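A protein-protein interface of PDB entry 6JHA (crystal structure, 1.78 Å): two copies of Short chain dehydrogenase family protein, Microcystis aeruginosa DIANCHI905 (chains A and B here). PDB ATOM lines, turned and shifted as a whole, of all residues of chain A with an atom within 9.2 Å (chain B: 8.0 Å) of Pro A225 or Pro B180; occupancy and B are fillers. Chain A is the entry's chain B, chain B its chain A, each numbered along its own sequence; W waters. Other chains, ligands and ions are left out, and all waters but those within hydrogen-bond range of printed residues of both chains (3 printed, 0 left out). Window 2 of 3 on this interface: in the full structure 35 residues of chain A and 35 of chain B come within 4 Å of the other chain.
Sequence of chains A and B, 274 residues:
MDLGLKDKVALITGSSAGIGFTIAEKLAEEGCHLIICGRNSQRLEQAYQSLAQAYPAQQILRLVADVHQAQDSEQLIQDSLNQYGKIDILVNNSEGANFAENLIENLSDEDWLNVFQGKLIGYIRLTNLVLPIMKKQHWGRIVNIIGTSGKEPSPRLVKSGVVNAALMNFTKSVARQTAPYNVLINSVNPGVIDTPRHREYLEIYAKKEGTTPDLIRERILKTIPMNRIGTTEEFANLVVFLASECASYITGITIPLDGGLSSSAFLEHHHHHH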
ATOM      1  N   ILE A 220      18.595   4.355 -18.830  1.00  0.00           N
ATOM      2  CA  ILE A 220      18.326   4.463 -17.380  1.00  0.00           C
ATOM      3  C   ILE A 220      19.358   3.683 -16.568  1.00  0.00           C
ATOM      4  O   ILE A 220      19.923   4.212 -15.591  1.00  0.00           O
ATOM      5  CB  ILE A 220      16.879   4.000 -17.083  1.00  0.00           C
ATOM      6  CG1 ILE A 220      15.954   5.022 -17.713  1.00  0.00           C
ATOM      7  CG2 ILE A 220      16.591   3.925 -15.596  1.00  0.00           C
ATOM      8  CD1 ILE A 220      14.479   4.758 -17.546  1.00  0.00           C
ATOM      9  N   LEU A 221      19.609   2.450 -16.994  1.00  0.00           N
ATOM     10  CA  LEU A 221      20.543   1.554 -16.324  1.00  0.00           C
ATOM     11  C   LEU A 221      21.960   2.114 -16.236  1.00  0.00           C
ATOM     12  O   LEU A 221      22.632   1.931 -15.212  1.00  0.00           O
ATOM     13  CB  LEU A 221      20.588   0.205 -16.999  1.00  0.00           C
ATOM     14  CG  LEU A 221      19.341  -0.696 -16.946  1.00  0.00           C
ATOM     15  CD1 LEU A 221      19.608  -1.936 -17.785  1.00  0.00           C
ATOM     16  CD2 LEU A 221      19.093  -1.070 -15.504  1.00  0.00           C
ATOM     17  N   LYS A 222      22.413   2.804 -17.277  1.00  0.00           N
ATOM     18  CA  LYS A 222      23.698   3.508 -17.203  1.00  0.00           C
ATOM     19  C   LYS A 222      23.731   4.614 -16.137  1.00  0.00           C
ATOM     20  O   LYS A 222      24.800   4.949 -15.609  1.00  0.00           O
ATOM     21  CB  LYS A 222      24.062   4.092 -18.581  1.00  0.00           C
ATOM     22  CG  LYS A 222      24.350   3.046 -19.639  1.00  0.00           C
ATOM     23  N   THR A 223      22.589   5.196 -15.790  1.00  0.00           N
ATOM     24  CA  THR A 223      22.575   6.220 -14.746  1.00  0.00           C
ATOM     25  C   THR A 223      22.537   5.673 -13.312  1.00  0.00           C
ATOM     26  O   THR A 223      22.794   6.399 -12.374  1.00  0.00           O
ATOM     27  CB  THR A 223      21.419   7.217 -14.880  1.00  0.00           C
ATOM     28  OG1 THR A 223      20.219   6.679 -14.291  1.00  0.00           O
ATOM     29  CG2 THR A 223      21.174   7.566 -16.363  1.00  0.00           C
ATOM     30  N   ILE A 224      22.125   4.425 -13.149  1.00  0.00           N
ATOM     31  CA  ILE A 224      21.996   3.849 -11.798  1.00  0.00           C
ATOM     32  C   ILE A 224      23.282   3.104 -11.424  1.00  0.00           C
ATOM     33  O   ILE A 224      23.708   2.201 -12.155  1.00  0.00           O
ATOM     34  CB  ILE A 224      20.810   2.837 -11.770  1.00  0.00           C
ATOM     35  CG1 ILE A 224      19.477   3.564 -12.123  1.00  0.00           C
ATOM     36  CG2 ILE A 224      20.725   2.140 -10.423  1.00  0.00           C
ATOM     37  CD1 ILE A 224      18.351   2.582 -12.401  1.00  0.00           C
ATOM     38  N   PRO A 225      23.950   3.486 -10.322  1.00  0.00           N
ATOM     39  CA  PRO A 225      25.226   2.773  -9.937  1.00  0.00           C
ATOM     40  C   PRO A 225      25.149   1.269  -9.858  1.00  0.00           C
ATOM     41  O   PRO A 225      26.067   0.566 -10.358  1.00  0.00           O
ATOM     42  CB  PRO A 225      25.626   3.475  -8.627  1.00  0.00           C
ATOM     43  CG  PRO A 225      25.129   4.894  -8.891  1.00  0.00           C
ATOM     44  CD  PRO A 225      23.746   4.672  -9.473  1.00  0.00           C
ATOM     45  N   MET A 226      24.036   0.738  -9.349  1.00  0.00           N
ATOM     46  CA  MET A 226      23.833  -0.679  -9.297  1.00  0.00           C
ATOM     47  C   MET A 226      23.642  -1.365 -10.641  1.00  0.00           C
ATOM     48  O   MET A 226      23.666  -2.596 -10.713  1.00  0.00           O
ATOM     49  CB  MET A 226      22.695  -1.018  -8.337  1.00  0.00           C
ATOM     50  CG  MET A 226      23.159  -0.905  -6.883  1.00  0.00           C
ATOM     51  SD  MET A 226      21.919  -1.598  -5.804  1.00  0.00           S
ATOM     52  CE  MET A 226      22.108  -0.622  -4.339  1.00  0.00           C
ATOM     53  N   ASN A 227      23.395  -0.580 -11.674  1.00  0.00           N
ATOM     54  CA  ASN A 227      23.192  -1.109 -13.023  1.00  0.00           C
ATOM     55  C   ASN A 227      22.000  -2.052 -13.111  1.00  0.00           C
ATOM     56  O   ASN A 227      22.027  -3.027 -13.844  1.00  0.00           O
ATOM     57  CB  ASN A 227      24.478  -1.779 -13.506  1.00  0.00           C
ATOM     58  CG  ASN A 227      24.526  -1.926 -15.004  1.00  0.00           C
ATOM     59  OD1 ASN A 227      23.867  -1.198 -15.724  1.00  0.00           O
ATOM     60  ND2 ASN A 227      25.275  -2.898 -15.474  1.00  0.00           N
ATOM     61  N   ARG A 228      20.944  -1.761 -12.360  1.00  0.00           N
ATOM     62  CA  ARG A 228      19.682  -2.507 -12.417  1.00  0.00           C
ATOM     63  C   ARG A 228      18.544  -1.710 -11.821  1.00  0.00           C
ATOM     64  O   ARG A 228      18.744  -0.792 -11.014  1.00  0.00           O
ATOM     65  CB  ARG A 228      19.759  -3.906 -11.825  1.00  0.00           C
ATOM     66  CG  ARG A 228      19.732  -3.963 -10.367  1.00  0.00           C
ATOM     67  CD  ARG A 228      19.656  -5.421  -9.865  1.00  0.00           C
ATOM     68  NE  ARG A 228      19.924  -5.292  -8.475  1.00  0.00           N
ATOM     69  CZ  ARG A 228      19.006  -5.057  -7.555  1.00  0.00           C
ATOM     70  NH1 ARG A 228      17.677  -5.058  -7.857  1.00  0.00           N
ATOM     71  NH2 ARG A 228      19.403  -4.921  -6.303  1.00  0.00           N
ATOM     72  N   ILE A 229      17.335  -2.016 -12.301  1.00  0.00           N
ATOM     73  CA  ILE A 229      16.125  -1.352 -11.860  1.00  0.00           C
ATOM     74  C   ILE A 229      15.616  -2.125 -10.634  1.00  0.00           C
ATOM     75  O   ILE A 229      15.761  -3.339 -10.594  1.00  0.00           O
ATOM     76  CB  ILE A 229      15.093  -1.283 -13.014  1.00  0.00           C
ATOM     77  CG1 ILE A 229      15.549  -0.135 -13.929  1.00  0.00           C
ATOM     78  CG2 ILE A 229      13.679  -0.997 -12.487  1.00  0.00           C
ATOM     79  CD1 ILE A 229      15.127  -0.228 -15.339  1.00  0.00           C
ATOM     80  N   ASP A 258      16.980   3.766  -4.201  1.00  0.00           N
ATOM     81  CA  ASP A 258      17.246   4.121  -5.604  1.00  0.00           C
ATOM     82  C   ASP A 258      18.479   3.507  -6.259  1.00  0.00           C
ATOM     83  O   ASP A 258      18.889   3.980  -7.311  1.00  0.00           O
ATOM     84  CB  ASP A 258      17.349   5.641  -5.688  1.00  0.00           C
ATOM     85  CG  ASP A 258      18.590   6.223  -4.967  1.00  0.00           C
ATOM     86  OD1 ASP A 258      18.682   7.458  -4.915  1.00  0.00           O
ATOM     87  OD2 ASP A 258      19.459   5.497  -4.427  1.00  0.00           O
ATOM     88  N   GLY A 259      19.072   2.477  -5.668  1.00  0.00           N
ATOM     89  CA  GLY A 259      20.181   1.803  -6.347  1.00  0.00           C
ATOM     90  C   GLY A 259      21.430   2.660  -6.480  1.00  0.00           C
ATOM     91  O   GLY A 259      22.325   2.369  -7.288  1.00  0.00           O
ATOM     92  N   GLY A 260      21.463   3.710  -5.693  1.00  0.00           N
ATOM     93  CA  GLY A 260      22.574   4.656  -5.686  1.00  0.00           C
ATOM     94  C   GLY A 260      22.370   5.869  -6.583  1.00  0.00           C
ATOM     95  O   GLY A 260      23.296   6.653  -6.759  1.00  0.00           O
ATOM     96  N   LEU A 261      21.186   6.031  -7.195  1.00  0.00           N
ATOM     97  CA  LEU A 261      20.946   7.164  -8.086  1.00  0.00           C
ATOM     98  C   LEU A 261      21.321   8.502  -7.435  1.00  0.00           C
ATOM     99  O   LEU A 261      21.930   9.359  -8.078  1.00  0.00           O
ATOM    100  CB  LEU A 261      19.479   7.179  -8.560  1.00  0.00           C
ATOM    101  CG  LEU A 261      19.079   7.822  -9.881  1.00  0.00           C
ATOM    102  CD1 LEU A 261      19.856   7.209 -11.041  1.00  0.00           C
ATOM    103  CD2 LEU A 261      17.577   7.627 -10.071  1.00  0.00           C
ATOM    104  N   SER A 262      21.007   8.694  -6.156  1.00  0.00           N
ATOM    105  CA  SER A 262      21.328   9.965  -5.453  1.00  0.00           C
ATOM    106  C   SER A 262      22.831  10.179  -5.287  1.00  0.00           C
ATOM    107  O   SER A 262      23.289  11.295  -5.087  1.00  0.00           O
ATOM    108  CB  SER A 262      20.683  10.017  -4.046  1.00  0.00           C
ATOM    109  OG  SER A 262      21.502   9.373  -3.062  1.00  0.00           O
ATOM    110  N   SER A 263      23.623   9.115  -5.328  1.00  0.00           N
ATOM    111  CA  SER A 263      25.079   9.267  -5.180  1.00  0.00           C
ATOM    112  C   SER A 263      25.717   9.667  -6.505  1.00  0.00           C
ATOM    113  O   SER A 263      26.886  10.035  -6.563  1.00  0.00           O
ATOM    114  CB  SER A 263      25.725   7.978  -4.660  1.00  0.00           C
ATOM    115  OG  SER A 263      25.870   7.012  -5.695  1.00  0.00           O
ATOM    116  N   SER A 264      24.911   9.603  -7.555  1.00  0.00           N
ATOM    117  CA  SER A 264      25.315   9.792  -8.930  1.00  0.00           C
ATOM    118  C   SER A 264      24.960  11.199  -9.471  1.00  0.00           C
ATOM    119  O   SER A 264      25.566  11.650 -10.427  1.00  0.00           O
ATOM    120  CB  SER A 264      24.604   8.731  -9.772  1.00  0.00           C
ATOM    121  OG  SER A 264      25.409   8.323 -10.843  1.00  0.00           O
ATOM    122  N   ALA A 265      23.966  11.868  -8.879  1.00  0.00           N
ATOM    123  CA  ALA A 265      23.592  13.267  -9.218  1.00  0.00           C
ATOM    124  C   ALA A 265      24.769  14.136  -9.702  1.00  0.00           C
ATOM    125  O   ALA A 265      25.841  14.129  -9.088  1.00  0.00           O
ATOM    126  CB  ALA A 265      22.913  13.934  -8.016  1.00  0.00           C
ATOM    127  N   LYS B 135      34.338  -7.214  -2.549  1.00  0.00           N
ATOM    128  CA  LYS B 135      34.189  -7.254  -4.033  1.00  0.00           C
ATOM    129  C   LYS B 135      34.412  -8.656  -4.540  1.00  0.00           C
ATOM    130  O   LYS B 135      33.719  -9.073  -5.452  1.00  0.00           O
ATOM    131  CB  LYS B 135      35.105  -6.270  -4.717  1.00  0.00           C
ATOM    132  CG  LYS B 135      34.715  -4.811  -4.549  1.00  0.00           C
ATOM    133  CD  LYS B 135      35.932  -3.996  -4.899  1.00  0.00           C
ATOM    134  CE  LYS B 135      35.659  -2.823  -5.779  1.00  0.00           C
ATOM    135  NZ  LYS B 135      36.888  -2.581  -6.612  1.00  0.00           N
ATOM    136  N   HIS B 138      31.250 -10.503  -4.112  1.00  0.00           N
ATOM    137  CA  HIS B 138      30.068  -9.810  -4.646  1.00  0.00           C
ATOM    138  C   HIS B 138      28.995  -9.669  -3.588  1.00  0.00           C
ATOM    139  O   HIS B 138      27.777  -9.821  -3.824  1.00  0.00           O
ATOM    140  CB  HIS B 138      29.502 -10.550  -5.867  1.00  0.00           C
ATOM    141  CG  HIS B 138      30.300 -10.348  -7.103  1.00  0.00           C
ATOM    142  ND1 HIS B 138      31.531 -10.940  -7.293  1.00  0.00           N
ATOM    143  CD2 HIS B 138      30.040  -9.653  -8.220  1.00  0.00           C
ATOM    144  CE1 HIS B 138      31.985 -10.635  -8.485  1.00  0.00           C
ATOM    145  NE2 HIS B 138      31.115  -9.831  -9.060  1.00  0.00           N
ATOM    146  N   LYS B 172      29.073   8.528  -0.085  1.00  0.00           N
ATOM    147  CA  LYS B 172      28.523   8.651  -1.442  1.00  0.00           C
ATOM    148  C   LYS B 172      29.456   8.265  -2.553  1.00  0.00           C
ATOM    149  O   LYS B 172      29.062   7.528  -3.474  1.00  0.00           O
ATOM    150  CB  LYS B 172      28.028  10.082  -1.718  1.00  0.00           C
ATOM    151  CG  LYS B 172      26.846  10.521  -0.909  1.00  0.00           C
ATOM    152  CD  LYS B 172      26.422  11.920  -1.364  1.00  0.00           C
ATOM    153  CE  LYS B 172      25.105  12.325  -0.728  1.00  0.00           C
ATOM    154  NZ  LYS B 172      24.508  13.463  -1.480  1.00  0.00           N
ATOM    155  N   VAL B 174      32.203   6.330  -2.363  1.00  0.00           N
ATOM    156  CA  VAL B 174      32.505   4.903  -2.401  1.00  0.00           C
ATOM    157  C   VAL B 174      31.298   4.090  -2.835  1.00  0.00           C
ATOM    158  O   VAL B 174      31.450   3.127  -3.661  1.00  0.00           O
ATOM    159  CB  VAL B 174      33.191   4.301  -1.127  1.00  0.00           C
ATOM    160  CG1 VAL B 174      32.705   4.887   0.171  1.00  0.00           C
ATOM    161  CG2 VAL B 174      33.068   2.770  -1.101  1.00  0.00           C
ATOM    162  N   ALA B 175      30.108   4.460  -2.361  1.00  0.00           N
ATOM    163  CA  ALA B 175      28.930   3.733  -2.758  1.00  0.00           C
ATOM    164  C   ALA B 175      28.786   3.678  -4.308  1.00  0.00           C
ATOM    165  O   ALA B 175      28.457   2.643  -4.877  1.00  0.00           O
ATOM    166  CB  ALA B 175      27.684   4.319  -2.104  1.00  0.00           C
ATOM    167  N   ARG B 176      28.982   4.804  -4.964  1.00  0.00           N
ATOM    168  CA  ARG B 176      28.880   4.891  -6.425  1.00  0.00           C
ATOM    169  C   ARG B 176      29.850   3.924  -7.105  1.00  0.00           C
ATOM    170  O   ARG B 176      29.517   3.251  -8.087  1.00  0.00           O
ATOM    171  CB  ARG B 176      29.163   6.348  -6.879  1.00  0.00           C
ATOM    172  CG  ARG B 176      28.870   6.652  -8.334  1.00  0.00           C
ATOM    173  CD  ARG B 176      29.017   8.145  -8.630  1.00  0.00           C
ATOM    174  NE  ARG B 176      30.344   8.657  -8.279  1.00  0.00           N
ATOM    175  N   GLN B 177      31.057   3.828  -6.592  1.00  0.00           N
ATOM    176  CA  GLN B 177      32.073   3.002  -7.218  1.00  0.00           C
ATOM    177  C   GLN B 177      31.845   1.500  -7.000  1.00  0.00           C
ATOM    178  O   GLN B 177      32.200   0.681  -7.870  1.00  0.00           O
ATOM    179  CB  GLN B 177      33.438   3.426  -6.657  1.00  0.00           C
ATOM    180  CG  GLN B 177      34.455   3.828  -7.689  1.00  0.00           C
ATOM    181  CD  GLN B 177      35.828   4.082  -7.078  1.00  0.00           C
ATOM    182  OE1 GLN B 177      36.576   3.148  -6.797  1.00  0.00           O
ATOM    183  NE2 GLN B 177      36.144   5.351  -6.839  1.00  0.00           N
ATOM    184  N   THR B 178      31.311   1.104  -5.836  1.00  0.00           N
ATOM    185  CA  THR B 178      31.232  -0.301  -5.425  1.00  0.00           C
ATOM    186  C   THR B 178      29.851  -0.947  -5.648  1.00  0.00           C
ATOM    187  O   THR B 178      29.685  -2.150  -5.493  1.00  0.00           O
ATOM    188  CB  THR B 178      31.663  -0.489  -3.957  1.00  0.00           C
ATOM    189  OG1 THR B 178      30.694   0.093  -3.048  1.00  0.00           O
ATOM    190  CG2 THR B 178      32.970   0.225  -3.736  1.00  0.00           C
ATOM    191  N   ALA B 179      28.859  -0.123  -5.973  1.00  0.00           N
ATOM    192  CA  ALA B 179      27.520  -0.597  -6.250  1.00  0.00           C
ATOM    193  C   ALA B 179      27.448  -1.724  -7.296  1.00  0.00           C
ATOM    194  O   ALA B 179      26.643  -2.663  -7.125  1.00  0.00           O
ATOM    195  CB  ALA B 179      26.630   0.580  -6.633  1.00  0.00           C
ATOM    196  N   PRO B 180      28.282  -1.659  -8.356  1.00  0.00           N
ATOM    197  CA  PRO B 180      28.263  -2.756  -9.365  1.00  0.00           C
ATOM    198  C   PRO B 180      28.749  -4.104  -8.847  1.00  0.00           C
ATOM    199  O   PRO B 180      28.630  -5.116  -9.568  1.00  0.00           O
ATOM    200  CB  PRO B 180      29.238  -2.256 -10.466  1.00  0.00           C
ATOM    201  CG  PRO B 180      29.473  -0.826 -10.205  1.00  0.00           C
ATOM    202  CD  PRO B 180      29.104  -0.522  -8.790  1.00  0.00           C
ATOM    203  N   TYR B 181      29.316  -4.133  -7.630  1.00  0.00           N
ATOM    204  CA  TYR B 181      29.778  -5.365  -6.989  1.00  0.00           C
ATOM    205  C   TYR B 181      28.879  -5.837  -5.850  1.00  0.00           C
ATOM    206  O   TYR B 181      29.223  -6.787  -5.088  1.00  0.00           O
ATOM    207  CB  TYR B 181      31.162  -5.141  -6.408  1.00  0.00           C
ATOM    208  CG  TYR B 181      32.187  -4.902  -7.437  1.00  0.00           C
ATOM    209  CD1 TYR B 181      32.903  -5.964  -7.960  1.00  0.00           C
ATOM    210  CD2 TYR B 181      32.420  -3.625  -7.948  1.00  0.00           C
ATOM    211  CE1 TYR B 181      33.874  -5.753  -8.931  1.00  0.00           C
ATOM    212  CE2 TYR B 181      33.393  -3.411  -8.909  1.00  0.00           C
ATOM    213  CZ  TYR B 181      34.099  -4.491  -9.406  1.00  0.00           C
ATOM    214  OH  TYR B 181      35.066  -4.302 -10.367  1.00  0.00           O
ATOM    215  N   ASN B 182      27.736  -5.178  -5.702  1.00  0.00           N
ATOM    216  CA  ASN B 182      26.795  -5.487  -4.613  1.00  0.00           C
ATOM    217  C   ASN B 182      27.492  -5.311  -3.247  1.00  0.00           C
ATOM    218  O   ASN B 182      27.260  -6.069  -2.290  1.00  0.00           O
ATOM    219  CB  ASN B 182      26.169  -6.884  -4.770  1.00  0.00           C
ATOM    220  CG  ASN B 182      25.214  -7.251  -3.618  1.00  0.00           C
ATOM    221  OD1 ASN B 182      24.451  -6.395  -3.114  1.00  0.00           O
ATOM    222  ND2 ASN B 182      25.241  -8.508  -3.187  1.00  0.00           N
ATOM    223  N   VAL B 183      28.334  -4.289  -3.194  1.00  0.00           N
ATOM    224  CA  VAL B 183      28.953  -3.808  -1.960  1.00  0.00           C
ATOM    225  C   VAL B 183      28.320  -2.454  -1.645  1.00  0.00           C
ATOM    226  O   VAL B 183      28.564  -1.448  -2.335  1.00  0.00           O
ATOM    227  CB  VAL B 183      30.468  -3.723  -2.104  1.00  0.00           C
ATOM    228  CG1 VAL B 183      31.092  -3.155  -0.838  1.00  0.00           C
ATOM    229  CG2 VAL B 183      31.040  -5.101  -2.407  1.00  0.00           C
ATOM    230  N   LEU B 184      27.436  -2.444  -0.657  1.00  0.00           N
ATOM    231  CA  LEU B 184      26.545  -1.294  -0.383  1.00  0.00           C
ATOM    232  C   LEU B 184      27.032  -0.579   0.848  1.00  0.00           C
ATOM    233  O   LEU B 184      27.449  -1.213   1.804  1.00  0.00           O
ATOM    234  CB  LEU B 184      25.104  -1.774  -0.187  1.00  0.00           C
ATOM    235  CG  LEU B 184      24.564  -2.751  -1.237  1.00  0.00           C
ATOM    236  CD1 LEU B 184      23.057  -2.957  -1.023  1.00  0.00           C
ATOM    237  CD2 LEU B 184      24.861  -2.198  -2.623  1.00  0.00           C
ATOM    238  N   TYR B 249      18.701  -2.704  -2.439  1.00  0.00           N
ATOM    239  CA  TYR B 249      18.662  -1.593  -3.398  1.00  0.00           C
ATOM    240  C   TYR B 249      18.960  -0.248  -2.732  1.00  0.00           C
ATOM    241  O   TYR B 249      18.631   0.805  -3.279  1.00  0.00           O
ATOM    242  CB  TYR B 249      17.313  -1.570  -4.103  1.00  0.00           C
ATOM    243  CG  TYR B 249      17.318  -0.954  -5.470  1.00  0.00           C
ATOM    244  CD1 TYR B 249      16.525   0.158  -5.777  1.00  0.00           C
ATOM    245  CD2 TYR B 249      18.184  -1.431  -6.452  1.00  0.00           C
ATOM    246  CE1 TYR B 249      16.559   0.700  -7.050  1.00  0.00           C
ATOM    247  CE2 TYR B 249      18.220  -0.889  -7.724  1.00  0.00           C
ATOM    248  CZ  TYR B 249      17.392   0.149  -8.034  1.00  0.00           C
ATOM    249  OH  TYR B 249      17.404   0.709  -9.332  1.00  0.00           O
ATOM    250  N   THR B 251      21.845   2.265  -1.214  1.00  0.00           N
ATOM    251  CA  THR B 251      23.248   2.583  -1.070  1.00  0.00           C
ATOM    252  C   THR B 251      23.505   4.068  -1.215  1.00  0.00           C
ATOM    253  O   THR B 251      22.785   4.772  -1.958  1.00  0.00           O
ATOM    254  CB  THR B 251      24.102   1.754  -2.028  1.00  0.00           C
ATOM    255  OG1 THR B 251      25.417   1.690  -1.571  1.00  0.00           O
ATOM    256  CG2 THR B 251      24.061   2.283  -3.486  1.00  0.00           C
HETATM  257  O   HOH W   1      19.138   4.180  -1.930  1.00  0.00           O
HETATM  258  O   HOH W   2      16.850   3.564  -9.147  1.00  0.00           O
HETATM  259  O   HOH W   3      21.686   6.854  -3.476  1.00  0.00           O
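Water W3 lies within hydrogen-bond range of the side-chain hydroxyl of Ser A262 (2.6 Å), the side-chain carboxylate of Asp A258 (2.8 Å) and the backbone carbonyl oxygen of Thr B251 (2.8 Å). Water W2 lies within hydrogen-bond range of the backbone carbonyl oxygen of Asp A258 (2.8 Å) and the side-chain hydroxyl of Tyr B249 (2.9 Å). Water W1 bridges OD2 of Asp A258 and N of Thr B251.
Pro B180 touches one residue of chain A. Printed residues of chain B within 4 Å of Gly A259: Tyr B249 (2.9 Å). Of the printed residues of chain B, Ile A229 touches Tyr B249 (3.5 Å). The nearest printed residue of chain B that does not touch Ile A229 is Ala B179 (10.7 Å).
The backbone NH (N) of Met A226 sits at hydrogen-bond distance from the backbone carbonyl oxygen (O) of Gly A259 (3.1 Å). N of Gly A260 lies within hydrogen-bond range of OD2 of Asp A258, 3.0 Å away. The side-chain carboxylate of Asp A258 sits at hydrogen-bond distance from the backbone NH of Leu A261. The backbone NH (N) of Ser A262 is in hydrogen-bond range of the side-chain carboxylate (OD1) of Asp A258 (2.9 Å). The backbone carbonyl oxygen of Gly A260 sits at hydrogen-bond distance from the side-chain hydroxyl of Ser A263, at 2.8 Å.
Ile A224 touches Tyr B249 (CD1 to OH, 3.7 Å). Pro A225 touches Arg B176 (CB to O, 3.9 Å). Ala B179 touches Pro A225 (CB to C, 3.6 Å). Pro A225 touches Pro B180. Met A226 touches Ala B179. Met A226 touches Thr B251. Tyr B249 touches Ile A229. Asp A258 touches Tyr B249 (C to CE1, 3.5 Å). Ser A263 touches Lys B172 (CB to O, 3.6 Å). Arg B176 touches Ser A263 (CD to O, 3.5 Å).
No position is printed for both chains.
The backbone carbonyl oxygen of Arg A228 sits at hydrogen-bond distance from the side-chain hydroxyl of Tyr B249 (2.6 Å). The backbone NH of Gly A259 sits at hydrogen-bond distance from the backbone carbonyl oxygen of Tyr B249 (2.9 Å).
Of the 16 printed residues of chain B, 7 touch a printed residue of chain A. Of the 18 printed residues of chain A, 9 touch a printed residue of chain B. Hydrophobic or aromatic side chains of chain A that line the printed part of chain B: Ile A224, Pro A225 and Met A226.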
